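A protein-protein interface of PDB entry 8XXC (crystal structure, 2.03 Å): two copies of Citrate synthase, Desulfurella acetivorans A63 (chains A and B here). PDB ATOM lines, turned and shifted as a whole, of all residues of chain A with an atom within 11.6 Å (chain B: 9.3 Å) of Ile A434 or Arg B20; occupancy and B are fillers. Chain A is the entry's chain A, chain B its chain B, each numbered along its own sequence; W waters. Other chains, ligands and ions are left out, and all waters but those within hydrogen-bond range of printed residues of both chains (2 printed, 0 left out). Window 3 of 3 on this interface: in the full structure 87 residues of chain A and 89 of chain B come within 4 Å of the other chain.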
ATOM      1  N   THR A  34     -14.364  -7.843 -17.591  1.00  0.00           N
ATOM      2  CA  THR A  34     -13.446  -8.968 -17.490  1.00  0.00           C
ATOM      3  C   THR A  34     -12.721  -9.013 -16.147  1.00  0.00           C
ATOM      4  O   THR A  34     -12.698  -8.036 -15.395  1.00  0.00           O
ATOM      5  CB  THR A  34     -12.360  -8.930 -18.554  1.00  0.00           C
ATOM      6  OG1 THR A  34     -11.509  -7.860 -18.132  1.00  0.00           O
ATOM      7  CG2 THR A  34     -12.929  -8.787 -19.950  1.00  0.00           C
ATOM      8  N   ILE A  35     -12.098 -10.165 -15.884  1.00  0.00           N
ATOM      9  CA  ILE A  35     -11.281 -10.376 -14.697  1.00  0.00           C
ATOM     10  C   ILE A  35     -10.292  -9.225 -14.544  1.00  0.00           C
ATOM     11  O   ILE A  35     -10.123  -8.673 -13.455  1.00  0.00           O
ATOM     12  CB  ILE A  35     -10.570 -11.740 -14.767  1.00  0.00           C
ATOM     13  CG1 ILE A  35     -11.606 -12.862 -14.672  1.00  0.00           C
ATOM     14  CG2 ILE A  35      -9.477 -11.847 -13.715  1.00  0.00           C
ATOM     15  CD1 ILE A  35     -11.044 -14.263 -14.604  1.00  0.00           C
ATOM     16  N   SER A  36      -9.645  -8.858 -15.646  1.00  0.00           N
ATOM     17  CA  SER A  36      -8.616  -7.836 -15.598  1.00  0.00           C
ATOM     18  C   SER A  36      -9.176  -6.527 -15.039  1.00  0.00           C
ATOM     19  O   SER A  36      -8.453  -5.807 -14.346  1.00  0.00           O
ATOM     20  CB  SER A  36      -8.034  -7.616 -16.942  1.00  0.00           C
ATOM     21  OG  SER A  36      -6.755  -7.054 -16.769  1.00  0.00           O
ATOM     22  N   ILE A  39     -10.167  -6.676 -11.168  1.00  0.00           N
ATOM     23  CA  ILE A  39      -8.957  -6.528 -10.388  1.00  0.00           C
ATOM     24  C   ILE A  39      -8.362  -5.126 -10.562  1.00  0.00           C
ATOM     25  O   ILE A  39      -7.796  -4.577  -9.612  1.00  0.00           O
ATOM     26  CB  ILE A  39      -7.938  -7.639 -10.734  1.00  0.00           C
ATOM     27  CG1 ILE A  39      -8.402  -9.012 -10.250  1.00  0.00           C
ATOM     28  CG2 ILE A  39      -6.570  -7.309 -10.151  1.00  0.00           C
ATOM     29  CD1 ILE A  39      -7.574 -10.159 -10.779  1.00  0.00           C
ATOM     30  N   THR A 424     -14.845 -12.697  -4.721  1.00  0.00           N
ATOM     31  CA  THR A 424     -13.596 -13.101  -4.118  1.00  0.00           C
ATOM     32  C   THR A 424     -12.631 -13.609  -5.192  1.00  0.00           C
ATOM     33  O   THR A 424     -13.026 -13.876  -6.328  1.00  0.00           O
ATOM     34  CB  THR A 424     -13.890 -14.196  -3.094  1.00  0.00           C
ATOM     35  OG1 THR A 424     -14.247 -15.355  -3.848  1.00  0.00           O
ATOM     36  CG2 THR A 424     -15.011 -13.825  -2.154  1.00  0.00           C
ATOM     37  N   THR A 425     -11.352 -13.733  -4.808  1.00  0.00           N
ATOM     38  CA  THR A 425     -10.324 -14.320  -5.646  1.00  0.00           C
ATOM     39  C   THR A 425     -10.717 -15.746  -6.025  1.00  0.00           C
ATOM     40  O   THR A 425     -10.419 -16.171  -7.121  1.00  0.00           O
ATOM     41  CB  THR A 425      -8.939 -14.313  -4.971  1.00  0.00           C
ATOM     42  OG1 THR A 425      -8.488 -13.004  -4.621  1.00  0.00           O
ATOM     43  CG2 THR A 425      -7.880 -14.929  -5.863  1.00  0.00           C
ATOM     44  N   ASP A 426     -11.307 -16.495  -5.092  1.00  0.00           N
ATOM     45  CA  ASP A 426     -11.720 -17.871  -5.323  1.00  0.00           C
ATOM     46  C   ASP A 426     -12.753 -17.919  -6.447  1.00  0.00           C
ATOM     47  O   ASP A 426     -12.756 -18.831  -7.270  1.00  0.00           O
ATOM     48  CB  ASP A 426     -12.339 -18.502  -4.072  1.00  0.00           C
ATOM     49  CG  ASP A 426     -11.364 -18.989  -3.003  1.00  0.00           C
ATOM     50  OD1 ASP A 426     -10.141 -18.964  -3.231  1.00  0.00           O
ATOM     51  OD2 ASP A 426     -11.836 -19.368  -1.925  1.00  0.00           O
ATOM     52  N   MET A 427     -13.660 -16.943  -6.442  1.00  0.00           N
ATOM     53  CA  MET A 427     -14.706 -16.865  -7.440  1.00  0.00           C
ATOM     54  C   MET A 427     -14.101 -16.568  -8.808  1.00  0.00           C
ATOM     55  O   MET A 427     -14.543 -17.145  -9.793  1.00  0.00           O
ATOM     56  CB  MET A 427     -15.749 -15.811  -7.057  1.00  0.00           C
ATOM     57  CG  MET A 427     -16.744 -16.311  -5.990  1.00  0.00           C
ATOM     58  SD  MET A 427     -17.668 -14.983  -5.087  1.00  0.00           S
ATOM     59  CE  MET A 427     -18.603 -14.310  -6.458  1.00  0.00           C
ATOM     60  N   LEU A 428     -13.113 -15.672  -8.876  1.00  0.00           N
ATOM     61  CA  LEU A 428     -12.453 -15.346 -10.133  1.00  0.00           C
ATOM     62  C   LEU A 428     -11.712 -16.564 -10.691  1.00  0.00           C
ATOM     63  O   LEU A 428     -11.676 -16.773 -11.903  1.00  0.00           O
ATOM     64  CB  LEU A 428     -11.438 -14.226  -9.928  1.00  0.00           C
ATOM     65  CG  LEU A 428     -11.996 -12.844  -9.600  1.00  0.00           C
ATOM     66  CD1 LEU A 428     -10.847 -11.899  -9.312  1.00  0.00           C
ATOM     67  CD2 LEU A 428     -12.843 -12.321 -10.732  1.00  0.00           C
ATOM     68  N   GLU A 429     -11.117 -17.352  -9.796  1.00  0.00           N
ATOM     69  CA  GLU A 429     -10.420 -18.557 -10.188  1.00  0.00           C
ATOM     70  C   GLU A 429     -11.392 -19.598 -10.741  1.00  0.00           C
ATOM     71  O   GLU A 429     -11.095 -20.240 -11.755  1.00  0.00           O
ATOM     72  CB  GLU A 429      -9.585 -19.049  -9.009  1.00  0.00           C
ATOM     73  CG  GLU A 429      -8.351 -18.182  -8.792  1.00  0.00           C
ATOM     74  CD  GLU A 429      -7.512 -18.630  -7.619  1.00  0.00           C
ATOM     75  OE1 GLU A 429      -8.049 -19.386  -6.823  1.00  0.00           O
ATOM     76  OE2 GLU A 429      -6.330 -18.255  -7.518  1.00  0.00           O
ATOM     77  N   LYS A 430     -12.548 -19.755 -10.084  1.00  0.00           N
ATOM     78  CA  LYS A 430     -13.593 -20.641 -10.570  1.00  0.00           C
ATOM     79  C   LYS A 430     -13.958 -20.261 -12.001  1.00  0.00           C
ATOM     80  O   LYS A 430     -13.929 -21.104 -12.896  1.00  0.00           O
ATOM     81  CB  LYS A 430     -14.781 -20.598  -9.602  1.00  0.00           C
ATOM     82  CG  LYS A 430     -16.020 -21.399  -9.983  1.00  0.00           C
ATOM     83  CD  LYS A 430     -17.029 -21.441  -8.830  1.00  0.00           C
ATOM     84  CE  LYS A 430     -18.374 -22.048  -9.156  1.00  0.00           C
ATOM     85  NZ  LYS A 430     -19.261 -22.039  -7.970  1.00  0.00           N
ATOM     86  N   TRP A 431     -14.281 -18.982 -12.217  1.00  0.00           N
ATOM     87  CA  TRP A 431     -14.650 -18.484 -13.541  1.00  0.00           C
ATOM     88  C   TRP A 431     -13.492 -18.529 -14.523  1.00  0.00           C
ATOM     89  O   TRP A 431     -13.724 -18.554 -15.731  1.00  0.00           O
ATOM     90  CB  TRP A 431     -15.177 -17.063 -13.440  1.00  0.00           C
ATOM     91  CG  TRP A 431     -16.407 -16.978 -12.594  1.00  0.00           C
ATOM     92  CD1 TRP A 431     -17.353 -17.947 -12.417  1.00  0.00           C
ATOM     93  CD2 TRP A 431     -16.805 -15.867 -11.776  1.00  0.00           C
ATOM     94  NE1 TRP A 431     -18.325 -17.508 -11.565  1.00  0.00           N
ATOM     95  CE2 TRP A 431     -18.024 -16.233 -11.159  1.00  0.00           C
ATOM     96  CE3 TRP A 431     -16.262 -14.601 -11.517  1.00  0.00           C
ATOM     97  CZ2 TRP A 431     -18.717 -15.367 -10.309  1.00  0.00           C
ATOM     98  CZ3 TRP A 431     -16.936 -13.758 -10.659  1.00  0.00           C
ATOM     99  CH2 TRP A 431     -18.150 -14.134 -10.073  1.00  0.00           C
ATOM    100  N   ALA A 432     -12.258 -18.499 -14.010  1.00  0.00           N
ATOM    101  CA  ALA A 432     -11.088 -18.646 -14.857  1.00  0.00           C
ATOM    102  C   ALA A 432     -10.918 -20.102 -15.313  1.00  0.00           C
ATOM    103  O   ALA A 432     -10.058 -20.373 -16.151  1.00  0.00           O
ATOM    104  CB  ALA A 432      -9.873 -18.192 -14.113  1.00  0.00           C
ATOM    105  N   GLY A 433     -11.674 -21.019 -14.679  1.00  0.00           N
ATOM    106  CA  GLY A 433     -11.726 -22.424 -15.043  1.00  0.00           C
ATOM    107  C   GLY A 433     -10.647 -23.290 -14.389  1.00  0.00           C
ATOM    108  O   GLY A 433     -10.477 -24.435 -14.793  1.00  0.00           O
ATOM    109  N   ILE A 434      -9.923 -22.778 -13.385  1.00  0.00           N
ATOM    110  CA  ILE A 434      -8.820 -23.530 -12.786  1.00  0.00           C
ATOM    111  C   ILE A 434      -9.293 -24.250 -11.513  1.00  0.00           C
ATOM    112  O   ILE A 434      -8.506 -24.513 -10.600  1.00  0.00           O
ATOM    113  CB  ILE A 434      -7.596 -22.614 -12.555  1.00  0.00           C
ATOM    114  CG1 ILE A 434      -7.870 -21.470 -11.581  1.00  0.00           C
ATOM    115  CG2 ILE A 434      -7.084 -22.067 -13.876  1.00  0.00           C
ATOM    116  CD1 ILE A 434      -6.744 -20.467 -11.469  1.00  0.00           C
ATOM    117  N   LYS A 435     -10.572 -24.651 -11.514  1.00  0.00           N
ATOM    118  CA  LYS A 435     -11.309 -24.989 -10.305  1.00  0.00           C
ATOM    119  C   LYS A 435     -10.989 -23.965  -9.213  1.00  0.00           C
ATOM    120  O   LYS A 435     -11.968 -23.405  -8.687  1.00  0.00           O
ATOM    121  CB  LYS A 435     -11.030 -26.424  -9.849  1.00  0.00           C
ATOM    122  CG  LYS A 435     -11.866 -27.478 -10.564  1.00  0.00           C
ATOM    123  CD  LYS A 435     -11.960 -28.786  -9.813  1.00  0.00           C
ATOM    124  CE  LYS A 435     -10.632 -29.502  -9.714  1.00  0.00           C
ATOM    125  NZ  LYS A 435     -10.691 -30.628  -8.754  1.00  0.00           N
ATOM    126  N   HIS B  14      -0.726 -15.164  -1.375  1.00  0.00           N
ATOM    127  CA  HIS B  14      -1.904 -14.761  -2.126  1.00  0.00           C
ATOM    128  C   HIS B  14      -1.497 -14.113  -3.446  1.00  0.00           C
ATOM    129  O   HIS B  14      -2.178 -14.293  -4.453  1.00  0.00           O
ATOM    130  CB  HIS B  14      -2.844 -13.877  -1.277  1.00  0.00           C
ATOM    131  CG  HIS B  14      -4.129 -13.522  -1.955  1.00  0.00           C
ATOM    132  ND1 HIS B  14      -4.190 -12.816  -3.145  1.00  0.00           N
ATOM    133  CD2 HIS B  14      -5.395 -13.819  -1.642  1.00  0.00           C
ATOM    134  CE1 HIS B  14      -5.451 -12.683  -3.519  1.00  0.00           C
ATOM    135  NE2 HIS B  14      -6.193 -13.288  -2.624  1.00  0.00           N
ATOM    136  N   ARG B  15      -0.383 -13.381  -3.435  1.00  0.00           N
ATOM    137  CA  ARG B  15       0.044 -12.556  -4.555  1.00  0.00           C
ATOM    138  C   ARG B  15       0.139 -13.308  -5.880  1.00  0.00           C
ATOM    139  O   ARG B  15      -0.162 -12.718  -6.926  1.00  0.00           O
ATOM    140  CB  ARG B  15       1.414 -11.943  -4.268  1.00  0.00           C
ATOM    141  CG  ARG B  15       1.308 -10.606  -3.573  1.00  0.00           C
ATOM    142  CD  ARG B  15       2.654 -10.055  -3.191  1.00  0.00           C
ATOM    143  NE  ARG B  15       2.449  -8.726  -2.639  1.00  0.00           N
ATOM    144  CZ  ARG B  15       3.370  -8.040  -1.973  1.00  0.00           C
ATOM    145  NH1 ARG B  15       3.056  -6.873  -1.437  1.00  0.00           N
ATOM    146  NH2 ARG B  15       4.587  -8.535  -1.820  1.00  0.00           N
ATOM    147  N   PRO B  16       0.692 -14.545  -5.918  1.00  0.00           N
ATOM    148  CA  PRO B  16       0.850 -15.286  -7.176  1.00  0.00           C
ATOM    149  C   PRO B  16      -0.489 -15.652  -7.794  1.00  0.00           C
ATOM    150  O   PRO B  16      -0.590 -15.736  -9.015  1.00  0.00           O
ATOM    151  CB  PRO B  16       1.622 -16.554  -6.763  1.00  0.00           C
ATOM    152  CG  PRO B  16       2.370 -16.110  -5.539  1.00  0.00           C
ATOM    153  CD  PRO B  16       1.369 -15.227  -4.815  1.00  0.00           C
ATOM    154  N   ARG B  17      -1.517 -15.821  -6.938  1.00  0.00           N
ATOM    155  CA  ARG B  17      -2.849 -16.112  -7.436  1.00  0.00           C
ATOM    156  C   ARG B  17      -3.398 -14.921  -8.235  1.00  0.00           C
ATOM    157  O   ARG B  17      -4.028 -15.136  -9.264  1.00  0.00           O
ATOM    158  CB  ARG B  17      -3.796 -16.473  -6.295  1.00  0.00           C
ATOM    159  CG  ARG B  17      -3.313 -17.618  -5.425  1.00  0.00           C
ATOM    160  CD  ARG B  17      -4.170 -17.695  -4.180  1.00  0.00           C
ATOM    161  NE  ARG B  17      -5.481 -18.264  -4.445  1.00  0.00           N
ATOM    162  CZ  ARG B  17      -6.544 -18.092  -3.673  1.00  0.00           C
ATOM    163  NH1 ARG B  17      -6.410 -17.450  -2.528  1.00  0.00           N
ATOM    164  NH2 ARG B  17      -7.735 -18.537  -4.052  1.00  0.00           N
ATOM    165  N   THR B  18      -3.150 -13.684  -7.763  1.00  0.00           N
ATOM    166  CA  THR B  18      -3.675 -12.473  -8.388  1.00  0.00           C
ATOM    167  C   THR B  18      -2.891 -12.246  -9.673  1.00  0.00           C
ATOM    168  O   THR B  18      -3.467 -11.888 -10.691  1.00  0.00           O
ATOM    169  CB  THR B  18      -3.591 -11.225  -7.469  1.00  0.00           C
ATOM    170  OG1 THR B  18      -4.244 -11.413  -6.214  1.00  0.00           O
ATOM    171  CG2 THR B  18      -4.214  -9.982  -8.074  1.00  0.00           C
ATOM    172  N   THR B  19      -1.569 -12.427  -9.597  1.00  0.00           N
ATOM    173  CA  THR B  19      -0.676 -12.239 -10.738  1.00  0.00           C
ATOM    174  C   THR B  19      -1.078 -13.180 -11.871  1.00  0.00           C
ATOM    175  O   THR B  19      -1.186 -12.757 -13.015  1.00  0.00           O
ATOM    176  CB  THR B  19       0.791 -12.436 -10.329  1.00  0.00           C
ATOM    177  OG1 THR B  19       1.093 -11.408  -9.397  1.00  0.00           O
ATOM    178  CG2 THR B  19       1.783 -12.376 -11.468  1.00  0.00           C
ATOM    179  N   ARG B  20      -1.349 -14.444 -11.522  1.00  0.00           N
ATOM    180  CA  ARG B  20      -1.786 -15.451 -12.481  1.00  0.00           C
ATOM    181  C   ARG B  20      -3.141 -15.103 -13.107  1.00  0.00           C
ATOM    182  O   ARG B  20      -3.363 -15.392 -14.280  1.00  0.00           O
ATOM    183  CB  ARG B  20      -1.884 -16.828 -11.816  1.00  0.00           C
ATOM    184  CG  ARG B  20      -2.245 -17.947 -12.784  1.00  0.00           C
ATOM    185  CD  ARG B  20      -2.286 -19.314 -12.127  1.00  0.00           C
ATOM    186  NE  ARG B  20      -2.444 -20.364 -13.125  1.00  0.00           N
ATOM    187  CZ  ARG B  20      -2.987 -21.558 -12.888  1.00  0.00           C
ATOM    188  NH1 ARG B  20      -3.317 -21.898 -11.656  1.00  0.00           N
ATOM    189  NH2 ARG B  20      -3.196 -22.403 -13.884  1.00  0.00           N
ATOM    190  N   LEU B  21      -4.077 -14.545 -12.330  1.00  0.00           N
ATOM    191  CA  LEU B  21      -5.364 -14.171 -12.891  1.00  0.00           C
ATOM    192  C   LEU B  21      -5.180 -13.082 -13.961  1.00  0.00           C
ATOM    193  O   LEU B  21      -5.837 -13.097 -14.994  1.00  0.00           O
ATOM    194  CB  LEU B  21      -6.297 -13.737 -11.749  1.00  0.00           C
ATOM    195  CG  LEU B  21      -6.964 -14.890 -10.992  1.00  0.00           C
ATOM    196  CD1 LEU B  21      -7.636 -14.406  -9.717  1.00  0.00           C
ATOM    197  CD2 LEU B  21      -7.963 -15.601 -11.870  1.00  0.00           C
ATOM    198  N   LEU B  22      -4.233 -12.167 -13.753  1.00  0.00           N
ATOM    199  CA  LEU B  22      -4.005 -11.070 -14.678  1.00  0.00           C
ATOM    200  C   LEU B  22      -3.176 -11.530 -15.878  1.00  0.00           C
ATOM    201  O   LEU B  22      -3.358 -11.046 -16.988  1.00  0.00           O
ATOM    202  CB  LEU B  22      -3.305  -9.933 -13.926  1.00  0.00           C
ATOM    203  CG  LEU B  22      -4.148  -9.262 -12.849  1.00  0.00           C
ATOM    204  CD1 LEU B  22      -3.364  -8.147 -12.148  1.00  0.00           C
ATOM    205  CD2 LEU B  22      -5.406  -8.710 -13.464  1.00  0.00           C
ATOM    206  N   SER B  23      -2.227 -12.414 -15.623  1.00  0.00           N
ATOM    207  CA  SER B  23      -1.288 -12.880 -16.638  1.00  0.00           C
ATOM    208  C   SER B  23      -1.989 -13.813 -17.641  1.00  0.00           C
ATOM    209  O   SER B  23      -2.011 -13.543 -18.839  1.00  0.00           O
ATOM    210  CB  SER B  23      -0.120 -13.533 -15.938  1.00  0.00           C
ATOM    211  OG  SER B  23       0.838 -14.020 -16.857  1.00  0.00           O
ATOM    212  N   GLU B  24      -2.643 -14.861 -17.138  1.00  0.00           N
ATOM    213  CA  GLU B  24      -3.226 -15.880 -17.997  1.00  0.00           C
ATOM    214  C   GLU B  24      -4.702 -15.627 -18.279  1.00  0.00           C
ATOM    215  O   GLU B  24      -5.181 -16.096 -19.302  1.00  0.00           O
ATOM    216  CB  GLU B  24      -3.158 -17.273 -17.363  1.00  0.00           C
ATOM    217  CG  GLU B  24      -1.770 -17.858 -17.163  1.00  0.00           C
ATOM    218  CD  GLU B  24      -1.830 -19.297 -16.662  1.00  0.00           C
ATOM    219  OE1 GLU B  24      -1.261 -19.584 -15.607  1.00  0.00           O
ATOM    220  OE2 GLU B  24      -2.504 -20.126 -17.307  1.00  0.00           O
ATOM    221  N   PHE B  25      -5.455 -14.966 -17.365  1.00  0.00           N
ATOM    222  CA  PHE B  25      -6.915 -15.043 -17.458  1.00  0.00           C
ATOM    223  C   PHE B  25      -7.580 -13.674 -17.480  1.00  0.00           C
ATOM    224  O   PHE B  25      -8.775 -13.588 -17.273  1.00  0.00           O
ATOM    225  CB  PHE B  25      -7.488 -15.868 -16.298  1.00  0.00           C
ATOM    226  CG  PHE B  25      -6.947 -17.271 -16.229  1.00  0.00           C
ATOM    227  CD1 PHE B  25      -7.194 -18.165 -17.265  1.00  0.00           C
ATOM    228  CD2 PHE B  25      -6.121 -17.666 -15.187  1.00  0.00           C
ATOM    229  CE1 PHE B  25      -6.643 -19.439 -17.244  1.00  0.00           C
ATOM    230  CE2 PHE B  25      -5.599 -18.952 -15.144  1.00  0.00           C
ATOM    231  CZ  PHE B  25      -5.874 -19.841 -16.166  1.00  0.00           C
ATOM    232  N   GLY B  26      -6.790 -12.630 -17.714  1.00  0.00           N
ATOM    233  CA  GLY B  26      -7.241 -11.252 -17.648  1.00  0.00           C
ATOM    234  C   GLY B  26      -8.497 -10.989 -18.468  1.00  0.00           C
ATOM    235  O   GLY B  26      -9.314 -10.165 -18.064  1.00  0.00           O
ATOM    236  N   ASN B  27      -8.670 -11.716 -19.581  1.00  0.00           N
ATOM    237  CA  ASN B  27      -9.647 -11.314 -20.591  1.00  0.00           C
ATOM    238  C   ASN B  27     -10.940 -12.110 -20.471  1.00  0.00           C
ATOM    239  O   ASN B  27     -11.861 -11.895 -21.270  1.00  0.00           O
ATOM    240  CB  ASN B  27      -9.101 -11.419 -22.019  1.00  0.00           C
ATOM    241  CG  ASN B  27      -8.079 -10.342 -22.329  1.00  0.00           C
ATOM    242  OD1 ASN B  27      -6.949 -10.635 -22.730  1.00  0.00           O
ATOM    243  ND2 ASN B  27      -8.463  -9.090 -22.144  1.00  0.00           N
ATOM    244  N   VAL B  28     -11.000 -12.997 -19.470  1.00  0.00           N
ATOM    245  CA  VAL B  28     -12.178 -13.811 -19.218  1.00  0.00           C
ATOM    246  C   VAL B  28     -13.318 -12.926 -18.745  1.00  0.00           C
ATOM    247  O   VAL B  28     -13.189 -12.183 -17.762  1.00  0.00           O
ATOM    248  CB  VAL B  28     -11.894 -14.864 -18.130  1.00  0.00           C
ATOM    249  CG1 VAL B  28     -13.154 -15.628 -17.757  1.00  0.00           C
ATOM    250  CG2 VAL B  28     -10.765 -15.795 -18.541  1.00  0.00           C
HETATM  251  O   HOH W   1      -4.788 -17.669  -9.539  1.00  0.00           O
HETATM  252  O   HOH W   2      -6.823 -11.160  -5.897  1.00  0.00           O
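No position is printed for both chains.
The backbone NH (N) of Ser A36 lies close to the side-chain hydroxyl (OG1) of Thr A34, 3.3 Å away. O of Glu A429 sits at hydrogen-bond distance from N of Ile A434. N of Asp A426 lies close to OG1 of Thr A424 (3.4 Å). The backbone carbonyl oxygen of Leu B21 is in hydrogen-bond range of the backbone NH of Gly B26 (2.9 Å). OG1 of Thr B18 lies close to ND1 of His B14, at 3.4 Å. OE1 of Glu B24 lies within salt-bridge range of NE of Arg B20, 2.9 Å away.
Water W1 bridges OE2 of Glu A429 (2.6 Å) and O of Arg B17 (2.7 Å). Water W2 lies within hydrogen-bond range of OG1 of Thr B18 (2.6 Å) and OG1 of Thr A425 (2.8 Å).
The side-chain carboxylate (OD1) of Asp A426 is in salt-bridge range of the guanidinium group (NH2) of Arg B17 (2.6 Å). A ring nitrogen (NE2) of His B14 sits at hydrogen-bond distance from the side-chain hydroxyl (OG1) of Thr A425, 3.1 Å away. The backbone carbonyl oxygen (O) of Gly B26 is in hydrogen-bond range of the side-chain hydroxyl (OG1) of Thr A34 (3.2 Å). The guanidinium group (NH2) of Arg B17 is in salt-bridge range of the side-chain carboxylate (OE1) of Glu A429 (2.9 Å). The backbone carbonyl oxygen (O) of Gly B26 is in hydrogen-bond range of the backbone NH (N) of Ser A36, at 2.8 Å. N of Ile A35 is in hydrogen-bond range of O of Val B28 (3.0 Å).
Of the 15 printed residues of chain B, 9 touch a printed residue of chain A. Printed residues of chain B that touch a printed residue of chain A: His B14, Arg B17, Arg B20, Leu B21, Leu B22, Phe B25, Gly B26, Asn B27 and Val B28. Hydrophobic or aromatic side chains of chain B that line the printed part of chain A: His B14, Leu B21, Leu B22, Phe B25 and Val B28. Of the 16 printed residues of chain A, 11 touch a printed residue of chain B. Among the printed residues, Asp or Glu carboxylates within 4 Å of a Lys or Arg side-chain nitrogen of the other chain: Asp A426 with Arg B17 (2.6 Å) and Glu A429 with Arg B17 (2.9 Å).
Among the printed residues, merely in contact across the chains: Thr A34 with Val B28 (3.2 Å), Ile A434 with Phe B25 (3.4 Å), Ile A35 with Gly B26 (3.5 Å), Thr A34 with Asn B27 (3.5 Å), Ile A35 with Phe B25 (3.6 Å), Trp A431 with Val B28 (3.6 Å), Ala A432 with Phe B25 (3.7 Å), Ile A434 with Arg B20 (3.7 Å), Ile A39 with Leu B22 (3.7 Å), Leu A428 with Leu B21 (3.8 Å), Thr A425 with Leu B21 (3.9 Å), Ile A39 with Leu B21 (3.9 Å), Ala A432 with Leu B21 (3.9 Å), Ser A36 with Leu B22 (3.9 Å) and Glu A429 with Leu B21 (3.95 Å).
Of the printed residues of chain B, Thr A34 touches Gly B26 (3.2 Å), Asn B27 (3.5 Å) and Val B28 (3.2 Å). Of the printed residues of chain B, Ile A35 touches Phe B25, Gly B26 and Val B28. Printed residues of chain B within 4 Å of Ile A39: Leu B21 and Leu B22. Ala A432 touches two residues of chain B. No residue of chain B comes within 4 Å of Gly A433. Of chain B, only Arg B20 (3.7 Å) and Phe B25 (3.4 Å) come within 4 Å of Ile A434. Lys A435 touches none of the printed residues of chain B. No residue of chain A comes within 4 Å of Pro B16. No residue of chain A comes within 4 Å of Thr B18. No residue of chain A comes within 4 Å of Thr B19. Of chain A, only Ile A434 comes within 4 Å of Arg B20. Of chain A, only Ile A39, Thr A425, Leu A428, Glu A429 and Ala A432 come within 4 Å of Leu B21. Of chain A, only Ser A36 (3.9 Å) and Ile A39 (3.7 Å) come within 4 Å of Leu B22. Ser B23 touches none of the printed residues of chain A. No residue of chain A comes within 4 Å of Glu B24. Phe B25 touches just these residues of chain A: Ile A35, Ala A432 and Ile A434. Of the printed residues of chain A, Gly B26 touches Thr A34 (3.2 Å), Ile A35 (3.5 Å) and Ser A36 (2.8 Å). Printed residues of chain A within 4 Å of Asn B27: Thr A34 (3.5 Å).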
